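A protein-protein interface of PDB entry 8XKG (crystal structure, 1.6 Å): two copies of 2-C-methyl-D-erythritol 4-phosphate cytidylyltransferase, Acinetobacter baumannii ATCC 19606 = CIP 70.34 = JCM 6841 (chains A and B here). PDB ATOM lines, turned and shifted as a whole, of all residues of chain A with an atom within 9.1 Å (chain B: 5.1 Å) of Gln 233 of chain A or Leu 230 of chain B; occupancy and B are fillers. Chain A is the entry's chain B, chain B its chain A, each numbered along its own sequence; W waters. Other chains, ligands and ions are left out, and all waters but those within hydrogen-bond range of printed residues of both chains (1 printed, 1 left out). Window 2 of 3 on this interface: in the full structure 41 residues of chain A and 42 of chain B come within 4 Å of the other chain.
Leu 230 of chain B touches its own counterpart, Leu 230 of chain A.
Leu 230 of chain A touches Ile 231 of chain B, but with the chains exchanged Ile 231 of chain A does not touch Leu 230 of chain B (5.6 Å).
Ile 231 of chain A touches Leu 227 of chain B, but with the chains exchanged Leu 227 of chain A does not touch Ile 231 of chain B (4.03 Å).
Ser 234 of chain A touches Leu 227 of chain B, but with the chains exchanged Leu 227 of chain A does not touch Ser 234 of chain B (7.5 Å).
Of the 8 pairs that touch across the chains among the printed residues, 3 have their exchanged pair printed and touching as well.
OG of Ser 234 of chain A sits at hydrogen-bond distance from O of Ile 231 of chain A (3.0 Å).
O of Ile 231 of chain B sits at hydrogen-bond distance from OG of Ser 234 of chain B (2.7 Å).
C of Leu 230 of chain A touches CD1 of Leu 227 of chain B, 3.9 Å away.
Leu 230 of chain A touches Leu 230 of chain B.
Leu 230 of chain A touches Ile 231 of chain B (CD1 to CG1, 3.9 Å).
OG of Ser 234 of chain B touches CD1 of Leu 230 of chain A (3.9 Å).
Ile 231 of chain A touches Leu 227 of chain B (CG1 to CD1, 3.9 Å).
Leu 230 of chain B touches Gln 233 of chain A (CD2 to OE1, 3.4 Å).
CA of Leu 227 of chain B touches CB of Ser 234 of chain A (3.96 Å).
Ser 234 of chain A touches Leu 230 of chain B.
Of the 17 printed residues of chain A, 4 touch a printed residue of chain B.
Hydrophobic or aromatic side chains of chain B within 4 Å of the printed part of chain A: Leu 227, Leu 230 and Ile 231.
Printed residues of chain B within 4 Å of Ser 234 of chain A: Leu 227 and Leu 230.
No residue of chain A comes within 4 Å of Arg 229 of chain B.
Of chain A, only Leu 230 (3.6 Å), Gln 233 (3.4 Å) and Ser 234 (3.6 Å) come within 4 Å of Leu 230 of chain B.
Printed residues of chain A within 4 Å of Ile 231 of chain B: Leu 230 (3.9 Å).
Printed residues of chain A within 4 Å of Ser 234 of chain B: Leu 230.
The nearest printed residue of chain B that does not touch Gln 233 of chain A is Arg 229 of chain B (5.2 Å).
The nearest residue of chain A that does not touch Leu 230 of chain B is Ile 231 of chain A (5.6 Å).
Water W1 bridges the side-chain carboxylate (OE2) of Glu 226 of chain A and the side-chain hydroxyl (OG) of Ser 234 of chain B.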
ATOM      1  N   ILE A  35       1.726  -6.281  16.534  1.00  0.00           N
ATOM      2  CA  ILE A  35       0.755  -6.894  17.404  1.00  0.00           C
ATOM      3  C   ILE A  35      -0.452  -5.945  17.301  1.00  0.00           C
ATOM      4  O   ILE A  35      -0.420  -4.870  17.763  1.00  0.00           O
ATOM      5  CB  ILE A  35       1.170  -6.995  18.828  1.00  0.00           C
ATOM      6  CG1 ILE A  35       2.284  -8.002  18.888  1.00  0.00           C
ATOM      7  CG2 ILE A  35       0.012  -7.555  19.601  1.00  0.00           C
ATOM      8  CD1 ILE A  35       2.945  -8.005  20.233  1.00  0.00           C
ATOM      9  N   GLN A  36      -1.459  -6.361  16.529  1.00  0.00           N
ATOM     10  CA  GLN A  36      -2.655  -5.545  16.211  1.00  0.00           C
ATOM     11  C   GLN A  36      -2.280  -4.259  15.428  1.00  0.00           C
ATOM     12  O   GLN A  36      -1.747  -4.354  14.323  1.00  0.00           O
ATOM     13  CB  GLN A  36      -3.576  -5.275  17.419  1.00  0.00           C
ATOM     14  CG  GLN A  36      -4.240  -6.521  17.982  1.00  0.00           C
ATOM     15  CD  GLN A  36      -5.485  -6.915  17.212  1.00  0.00           C
ATOM     16  OE1 GLN A  36      -5.765  -6.372  16.143  1.00  0.00           O
ATOM     17  NE2 GLN A  36      -6.239  -7.865  17.752  1.00  0.00           N
ATOM     18  N   HIS A  43       4.440  -1.156  21.580  1.00  0.00           N
ATOM     19  CA  HIS A  43       3.801  -1.739  22.756  1.00  0.00           C
ATOM     20  C   HIS A  43       4.729  -1.698  23.960  1.00  0.00           C
ATOM     21  O   HIS A  43       4.306  -1.360  25.072  1.00  0.00           O
ATOM     22  CB  HIS A  43       3.377  -3.178  22.473  1.00  0.00           C
ATOM     23  CG  HIS A  43       2.196  -3.296  21.563  1.00  0.00           C
ATOM     24  ND1 HIS A  43       0.910  -3.020  21.975  1.00  0.00           N
ATOM     25  CD2 HIS A  43       2.103  -3.675  20.267  1.00  0.00           C
ATOM     26  CE1 HIS A  43       0.077  -3.216  20.968  1.00  0.00           C
ATOM     27  NE2 HIS A  43       0.776  -3.613  19.919  1.00  0.00           N
ATOM     28  N   ARG A  47       4.096   0.374  27.477  1.00  0.00           N
ATOM     29  CA  ARG A  47       4.070  -0.265  28.785  1.00  0.00           C
ATOM     30  C   ARG A  47       5.076   0.386  29.731  1.00  0.00           C
ATOM     31  O   ARG A  47       4.739   0.728  30.871  1.00  0.00           O
ATOM     32  CB  ARG A  47       4.332  -1.761  28.632  1.00  0.00           C
ATOM     33  CG  ARG A  47       4.224  -2.538  29.915  1.00  0.00           C
ATOM     34  CD  ARG A  47       2.855  -2.398  30.588  1.00  0.00           C
ATOM     35  NE  ARG A  47       1.720  -2.790  29.755  1.00  0.00           N
ATOM     36  CZ  ARG A  47       1.274  -4.033  29.616  1.00  0.00           C
ATOM     37  NH1 ARG A  47       1.877  -5.056  30.199  1.00  0.00           N
ATOM     38  NH2 ARG A  47       0.185  -4.253  28.884  1.00  0.00           N
ATOM     39  N   CYS A 117       5.092  -7.454  27.190  1.00  0.00           N
ATOM     40  CA  CYS A 117       4.049  -7.913  28.098  1.00  0.00           C
ATOM     41  C   CYS A 117       4.405  -7.745  29.567  1.00  0.00           C
ATOM     42  O   CYS A 117       3.615  -8.150  30.426  1.00  0.00           O
ATOM     43  CB  CYS A 117       3.709  -9.380  27.818  1.00  0.00           C
ATOM     44  SG  CYS A 117       3.379  -9.760  26.081  1.00  0.00           S
ATOM     45  N   ASP A 215       4.624 -14.932  31.807  1.00  0.00           N
ATOM     46  CA  ASP A 215       4.118 -14.339  30.576  1.00  0.00           C
ATOM     47  C   ASP A 215       4.874 -13.078  30.166  1.00  0.00           C
ATOM     48  O   ASP A 215       4.440 -12.387  29.239  1.00  0.00           O
ATOM     49  CB  ASP A 215       2.610 -14.060  30.681  1.00  0.00           C
ATOM     50  CG  ASP A 215       2.261 -12.927  31.635  1.00  0.00           C
ATOM     51  OD1 ASP A 215       3.136 -12.426  32.370  1.00  0.00           O
ATOM     52  OD2 ASP A 215       1.074 -12.535  31.643  1.00  0.00           O
ATOM     53  N   LEU A 225       4.594 -13.787  18.310  1.00  0.00           N
ATOM     54  CA  LEU A 225       3.778 -12.587  18.154  1.00  0.00           C
ATOM     55  C   LEU A 225       2.327 -12.863  18.512  1.00  0.00           C
ATOM     56  O   LEU A 225       1.687 -12.064  19.206  1.00  0.00           O
ATOM     57  CB  LEU A 225       3.880 -12.062  16.725  1.00  0.00           C
ATOM     58  CG  LEU A 225       5.249 -11.521  16.338  1.00  0.00           C
ATOM     59  CD1 LEU A 225       5.420 -11.552  14.834  1.00  0.00           C
ATOM     60  CD2 LEU A 225       5.390 -10.113  16.869  1.00  0.00           C
ATOM     61  N   GLU A 226       1.783 -13.982  18.032  1.00  0.00           N
ATOM     62  CA  GLU A 226       0.417 -14.338  18.389  1.00  0.00           C
ATOM     63  C   GLU A 226       0.289 -14.543  19.892  1.00  0.00           C
ATOM     64  O   GLU A 226      -0.639 -14.025  20.523  1.00  0.00           O
ATOM     65  CB  GLU A 226      -0.010 -15.597  17.642  1.00  0.00           C
ATOM     66  CG  GLU A 226      -1.406 -16.058  17.995  1.00  0.00           C
ATOM     67  CD  GLU A 226      -1.739 -17.399  17.389  1.00  0.00           C
ATOM     68  OE1 GLU A 226      -2.525 -17.430  16.421  1.00  0.00           O
ATOM     69  OE2 GLU A 226      -1.214 -18.422  17.879  1.00  0.00           O
ATOM     70  N   LEU A 227       1.233 -15.275  20.487  1.00  0.00           N
ATOM     71  CA  LEU A 227       1.174 -15.515  21.925  1.00  0.00           C
ATOM     72  C   LEU A 227       1.239 -14.207  22.702  1.00  0.00           C
ATOM     73  O   LEU A 227       0.483 -14.010  23.662  1.00  0.00           O
ATOM     74  CB  LEU A 227       2.305 -16.448  22.352  1.00  0.00           C
ATOM     75  CG  LEU A 227       2.350 -16.766  23.847  1.00  0.00           C
ATOM     76  CD1 LEU A 227       1.020 -17.345  24.331  1.00  0.00           C
ATOM     77  CD2 LEU A 227       3.500 -17.706  24.153  1.00  0.00           C
ATOM     78  N   ALA A 228       2.129 -13.296  22.298  1.00  0.00           N
ATOM     79  CA  ALA A 228       2.199 -11.993  22.952  1.00  0.00           C
ATOM     80  C   ALA A 228       0.886 -11.234  22.809  1.00  0.00           C
ATOM     81  O   ALA A 228       0.451 -10.552  23.744  1.00  0.00           O
ATOM     82  CB  ALA A 228       3.356 -11.175  22.380  1.00  0.00           C
ATOM     83  N   ARG A 229       0.248 -11.327  21.641  1.00  0.00           N
ATOM     84  CA  ARG A 229      -1.062 -10.710  21.469  1.00  0.00           C
ATOM     85  C   ARG A 229      -2.058 -11.251  22.485  1.00  0.00           C
ATOM     86  O   ARG A 229      -2.761 -10.483  23.155  1.00  0.00           O
ATOM     87  CB  ARG A 229      -1.570 -10.945  20.047  1.00  0.00           C
ATOM     88  CG  ARG A 229      -2.862 -10.224  19.744  1.00  0.00           C
ATOM     89  CD  ARG A 229      -3.280 -10.438  18.303  1.00  0.00           C
ATOM     90  NE  ARG A 229      -3.595 -11.833  18.015  1.00  0.00           N
ATOM     91  CZ  ARG A 229      -4.660 -12.477  18.474  1.00  0.00           C
ATOM     92  NH1 ARG A 229      -5.519 -11.897  19.296  1.00  0.00           N
ATOM     93  NH2 ARG A 229      -4.871 -13.735  18.096  1.00  0.00           N
ATOM     94  N   LEU A 230      -2.113 -12.576  22.633  1.00  0.00           N
ATOM     95  CA  LEU A 230      -3.054 -13.173  23.575  1.00  0.00           C
ATOM     96  C   LEU A 230      -2.692 -12.832  25.014  1.00  0.00           C
ATOM     97  O   LEU A 230      -3.583 -12.583  25.836  1.00  0.00           O
ATOM     98  CB  LEU A 230      -3.107 -14.687  23.375  1.00  0.00           C
ATOM     99  CG  LEU A 230      -3.462 -15.177  21.970  1.00  0.00           C
ATOM    100  CD1 LEU A 230      -3.415 -16.694  21.923  1.00  0.00           C
ATOM    101  CD2 LEU A 230      -4.831 -14.667  21.542  1.00  0.00           C
ATOM    102  N   ILE A 231      -1.395 -12.793  25.336  1.00  0.00           N
ATOM    103  CA  ILE A 231      -0.987 -12.436  26.693  1.00  0.00           C
ATOM    104  C   ILE A 231      -1.477 -11.037  27.028  1.00  0.00           C
ATOM    105  O   ILE A 231      -2.085 -10.806  28.080  1.00  0.00           O
ATOM    106  CB  ILE A 231       0.540 -12.530  26.854  1.00  0.00           C
ATOM    107  CG1 ILE A 231       1.014 -13.981  26.861  1.00  0.00           C
ATOM    108  CG2 ILE A 231       0.966 -11.846  28.143  1.00  0.00           C
ATOM    109  CD1 ILE A 231       2.511 -14.122  26.648  1.00  0.00           C
ATOM    110  N   LEU A 232      -1.227 -10.084  26.126  1.00  0.00           N
ATOM    111  CA  LEU A 232      -1.688  -8.721  26.350  1.00  0.00           C
ATOM    112  C   LEU A 232      -3.195  -8.699  26.561  1.00  0.00           C
ATOM    113  O   LEU A 232      -3.701  -7.977  27.427  1.00  0.00           O
ATOM    114  CB  LEU A 232      -1.291  -7.837  25.168  1.00  0.00           C
ATOM    115  CG  LEU A 232       0.204  -7.530  25.029  1.00  0.00           C
ATOM    116  CD1 LEU A 232       0.485  -6.790  23.732  1.00  0.00           C
ATOM    117  CD2 LEU A 232       0.710  -6.736  26.220  1.00  0.00           C
ATOM    118  N   GLN A 233      -3.926  -9.507  25.790  1.00  0.00           N
ATOM    119  CA  GLN A 233      -5.367  -9.603  25.984  1.00  0.00           C
ATOM    120  C   GLN A 233      -5.706 -10.328  27.282  1.00  0.00           C
ATOM    121  O   GLN A 233      -6.638  -9.934  27.993  1.00  0.00           O
ATOM    122  CB  GLN A 233      -6.007 -10.317  24.797  1.00  0.00           C
ATOM    123  CG  GLN A 233      -7.526 -10.361  24.837  1.00  0.00           C
ATOM    124  CD  GLN A 233      -8.113 -11.259  23.762  1.00  0.00           C
ATOM    125  OE1 GLN A 233      -9.229 -11.754  23.894  1.00  0.00           O
ATOM    126  NE2 GLN A 233      -7.354 -11.488  22.704  1.00  0.00           N
ATOM    127  N   SER A 234      -5.005 -11.394  27.648  1.00  0.00           N
ATOM    128  CA  SER A 234      -5.263 -12.149  28.875  1.00  0.00           C
ATOM    129  C   SER A 234      -5.007 -11.401  30.127  1.00  0.00           C
ATOM    130  O   SER A 234      -5.464 -11.733  31.169  1.00  0.00           O
ATOM    131  CB  SER A 234      -4.449 -13.454  28.925  1.00  0.00           C
ATOM    132  OG  SER A 234      -3.186 -13.193  29.479  1.00  0.00           O
ATOM    133  N   GLN A 235      -4.245 -10.355  30.016  1.00  0.00           N
ATOM    134  CA  GLN A 235      -3.911  -9.503  31.126  1.00  0.00           C
ATOM    135  C   GLN A 235      -5.083  -8.497  31.323  1.00  0.00           C
ATOM    136  O   GLN A 235      -5.841  -8.289  30.422  1.00  0.00           O
ATOM    137  CB  GLN A 235      -2.602  -8.733  30.803  1.00  0.00           C
ATOM    138  CG  GLN A 235      -1.334  -9.405  31.311  1.00  0.00           C
ATOM    139  CD  GLN A 235      -0.052  -8.779  30.789  1.00  0.00           C
ATOM    140  OE1 GLN A 235      -0.030  -7.754  30.184  1.00  0.00           O
ATOM    141  NE2 GLN A 235       0.964  -9.464  30.980  1.00  0.00           N
ATOM    142  N   GLU B 226      -6.926 -18.181  32.100  1.00  0.00           N
ATOM    143  CA  GLU B 226      -7.446 -17.293  31.066  1.00  0.00           C
ATOM    144  C   GLU B 226      -6.604 -17.359  29.797  1.00  0.00           C
ATOM    145  O   GLU B 226      -7.148 -17.411  28.687  1.00  0.00           O
ATOM    146  CB  GLU B 226      -7.509 -15.865  31.607  1.00  0.00           C
ATOM    147  CG  GLU B 226      -8.088 -14.807  30.672  1.00  0.00           C
ATOM    148  CD  GLU B 226      -9.468 -15.144  30.128  1.00  0.00           C
ATOM    149  OE1 GLU B 226     -10.191 -15.957  30.741  1.00  0.00           O
ATOM    150  OE2 GLU B 226      -9.841 -14.558  29.090  1.00  0.00           O
ATOM    151  N   LEU B 227      -5.277 -17.339  29.938  1.00  0.00           N
ATOM    152  CA  LEU B 227      -4.415 -17.408  28.762  1.00  0.00           C
ATOM    153  C   LEU B 227      -4.638 -18.704  27.994  1.00  0.00           C
ATOM    154  O   LEU B 227      -4.713 -18.696  26.759  1.00  0.00           O
ATOM    155  CB  LEU B 227      -2.949 -17.266  29.168  1.00  0.00           C
ATOM    156  CG  LEU B 227      -1.918 -17.301  28.038  1.00  0.00           C
ATOM    157  CD1 LEU B 227      -2.154 -16.184  27.028  1.00  0.00           C
ATOM    158  CD2 LEU B 227      -0.519 -17.213  28.621  1.00  0.00           C
ATOM    159  N   ALA B 228      -4.749 -19.828  28.706  1.00  0.00           N
ATOM    160  CA  ALA B 228      -5.036 -21.093  28.039  1.00  0.00           C
ATOM    161  C   ALA B 228      -6.372 -21.037  27.312  1.00  0.00           C
ATOM    162  O   ALA B 228      -6.498 -21.547  26.192  1.00  0.00           O
ATOM    163  CB  ALA B 228      -5.021 -22.239  29.050  1.00  0.00           C
ATOM    164  N   ARG B 229      -7.377 -20.405  27.925  1.00  0.00           N
ATOM    165  CA  ARG B 229      -8.655 -20.219  27.246  1.00  0.00           C
ATOM    166  C   ARG B 229      -8.465 -19.480  25.929  1.00  0.00           C
ATOM    167  O   ARG B 229      -9.016 -19.875  24.894  1.00  0.00           O
ATOM    168  CB  ARG B 229      -9.634 -19.469  28.152  1.00  0.00           C
ATOM    169  CG  ARG B 229     -11.041 -19.364  27.581  1.00  0.00           C
ATOM    170  CD  ARG B 229     -11.927 -18.456  28.423  1.00  0.00           C
ATOM    171  NE  ARG B 229     -11.606 -17.042  28.273  1.00  0.00           N
ATOM    172  CZ  ARG B 229     -11.935 -16.301  27.223  1.00  0.00           C
ATOM    173  NH1 ARG B 229     -12.563 -16.821  26.180  1.00  0.00           N
ATOM    174  NH2 ARG B 229     -11.623 -15.008  27.217  1.00  0.00           N
ATOM    175  N   LEU B 230      -7.676 -18.405  25.946  1.00  0.00           N
ATOM    176  CA  LEU B 230      -7.451 -17.641  24.724  1.00  0.00           C
ATOM    177  C   LEU B 230      -6.660 -18.445  23.699  1.00  0.00           C
ATOM    178  O   LEU B 230      -6.922 -18.350  22.495  1.00  0.00           O
ATOM    179  CB  LEU B 230      -6.741 -16.332  25.055  1.00  0.00           C
ATOM    180  CG  LEU B 230      -7.584 -15.383  25.905  1.00  0.00           C
ATOM    181  CD1 LEU B 230      -6.766 -14.187  26.337  1.00  0.00           C
ATOM    182  CD2 LEU B 230      -8.819 -14.941  25.137  1.00  0.00           C
ATOM    183  N   ILE B 231      -5.681 -19.233  24.150  1.00  0.00           N
ATOM    184  CA  ILE B 231      -4.914 -20.062  23.221  1.00  0.00           C
ATOM    185  C   ILE B 231      -5.815 -21.097  22.558  1.00  0.00           C
ATOM    186  O   ILE B 231      -5.809 -21.259  21.332  1.00  0.00           O
ATOM    187  CB  ILE B 231      -3.726 -20.725  23.939  1.00  0.00           C
ATOM    188  CG1 ILE B 231      -2.692 -19.675  24.345  1.00  0.00           C
ATOM    189  CG2 ILE B 231      -3.082 -21.761  23.039  1.00  0.00           C
ATOM    190  CD1 ILE B 231      -1.654 -20.197  25.310  1.00  0.00           C
ATOM    191  N   LEU B 232      -6.597 -21.824  23.364  1.00  0.00           N
ATOM    192  CA  LEU B 232      -7.499 -22.836  22.818  1.00  0.00           C
ATOM    193  C   LEU B 232      -8.484 -22.229  21.830  1.00  0.00           C
ATOM    194  O   LEU B 232      -8.768 -22.816  20.779  1.00  0.00           O
ATOM    195  CB  LEU B 232      -8.255 -23.525  23.950  1.00  0.00           C
ATOM    196  CG  LEU B 232      -7.412 -24.409  24.860  1.00  0.00           C
ATOM    197  CD1 LEU B 232      -8.282 -24.983  25.962  1.00  0.00           C
ATOM    198  CD2 LEU B 232      -6.759 -25.509  24.043  1.00  0.00           C
ATOM    199  N   GLN B 233      -8.944 -21.032  22.105  1.00  0.00           N
ATOM    200  CA  GLN B 233      -9.888 -20.342  21.246  1.00  0.00           C
ATOM    201  C   GLN B 233      -9.252 -19.946  19.955  1.00  0.00           C
ATOM    202  O   GLN B 233      -9.860 -19.974  18.949  1.00  0.00           O
ATOM    203  CB  GLN B 233     -10.549 -19.154  21.941  1.00  0.00           C
ATOM    204  CG  GLN B 233     -11.475 -18.416  20.996  1.00  0.00           C
ATOM    205  CD  GLN B 233     -12.055 -17.121  21.445  1.00  0.00           C
ATOM    206  OE1 GLN B 233     -13.161 -16.781  20.939  1.00  0.00           O
ATOM    207  NE2 GLN B 233     -11.353 -16.336  22.303  1.00  0.00           N
ATOM    208  N   SER B 234      -7.982 -19.595  19.994  1.00  0.00           N
ATOM    209  CA  SER B 234      -7.241 -19.279  18.777  1.00  0.00           C
ATOM    210  C   SER B 234      -6.903 -20.515  17.947  1.00  0.00           C
ATOM    211  O   SER B 234      -6.537 -20.374  16.776  1.00  0.00           O
ATOM    212  CB  SER B 234      -5.947 -18.544  19.121  1.00  0.00           C
ATOM    213  OG  SER B 234      -4.958 -19.451  19.580  1.00  0.00           O
HETATM  214  O   HOH W   1      -2.856 -20.550  18.021  1.00  0.00           O
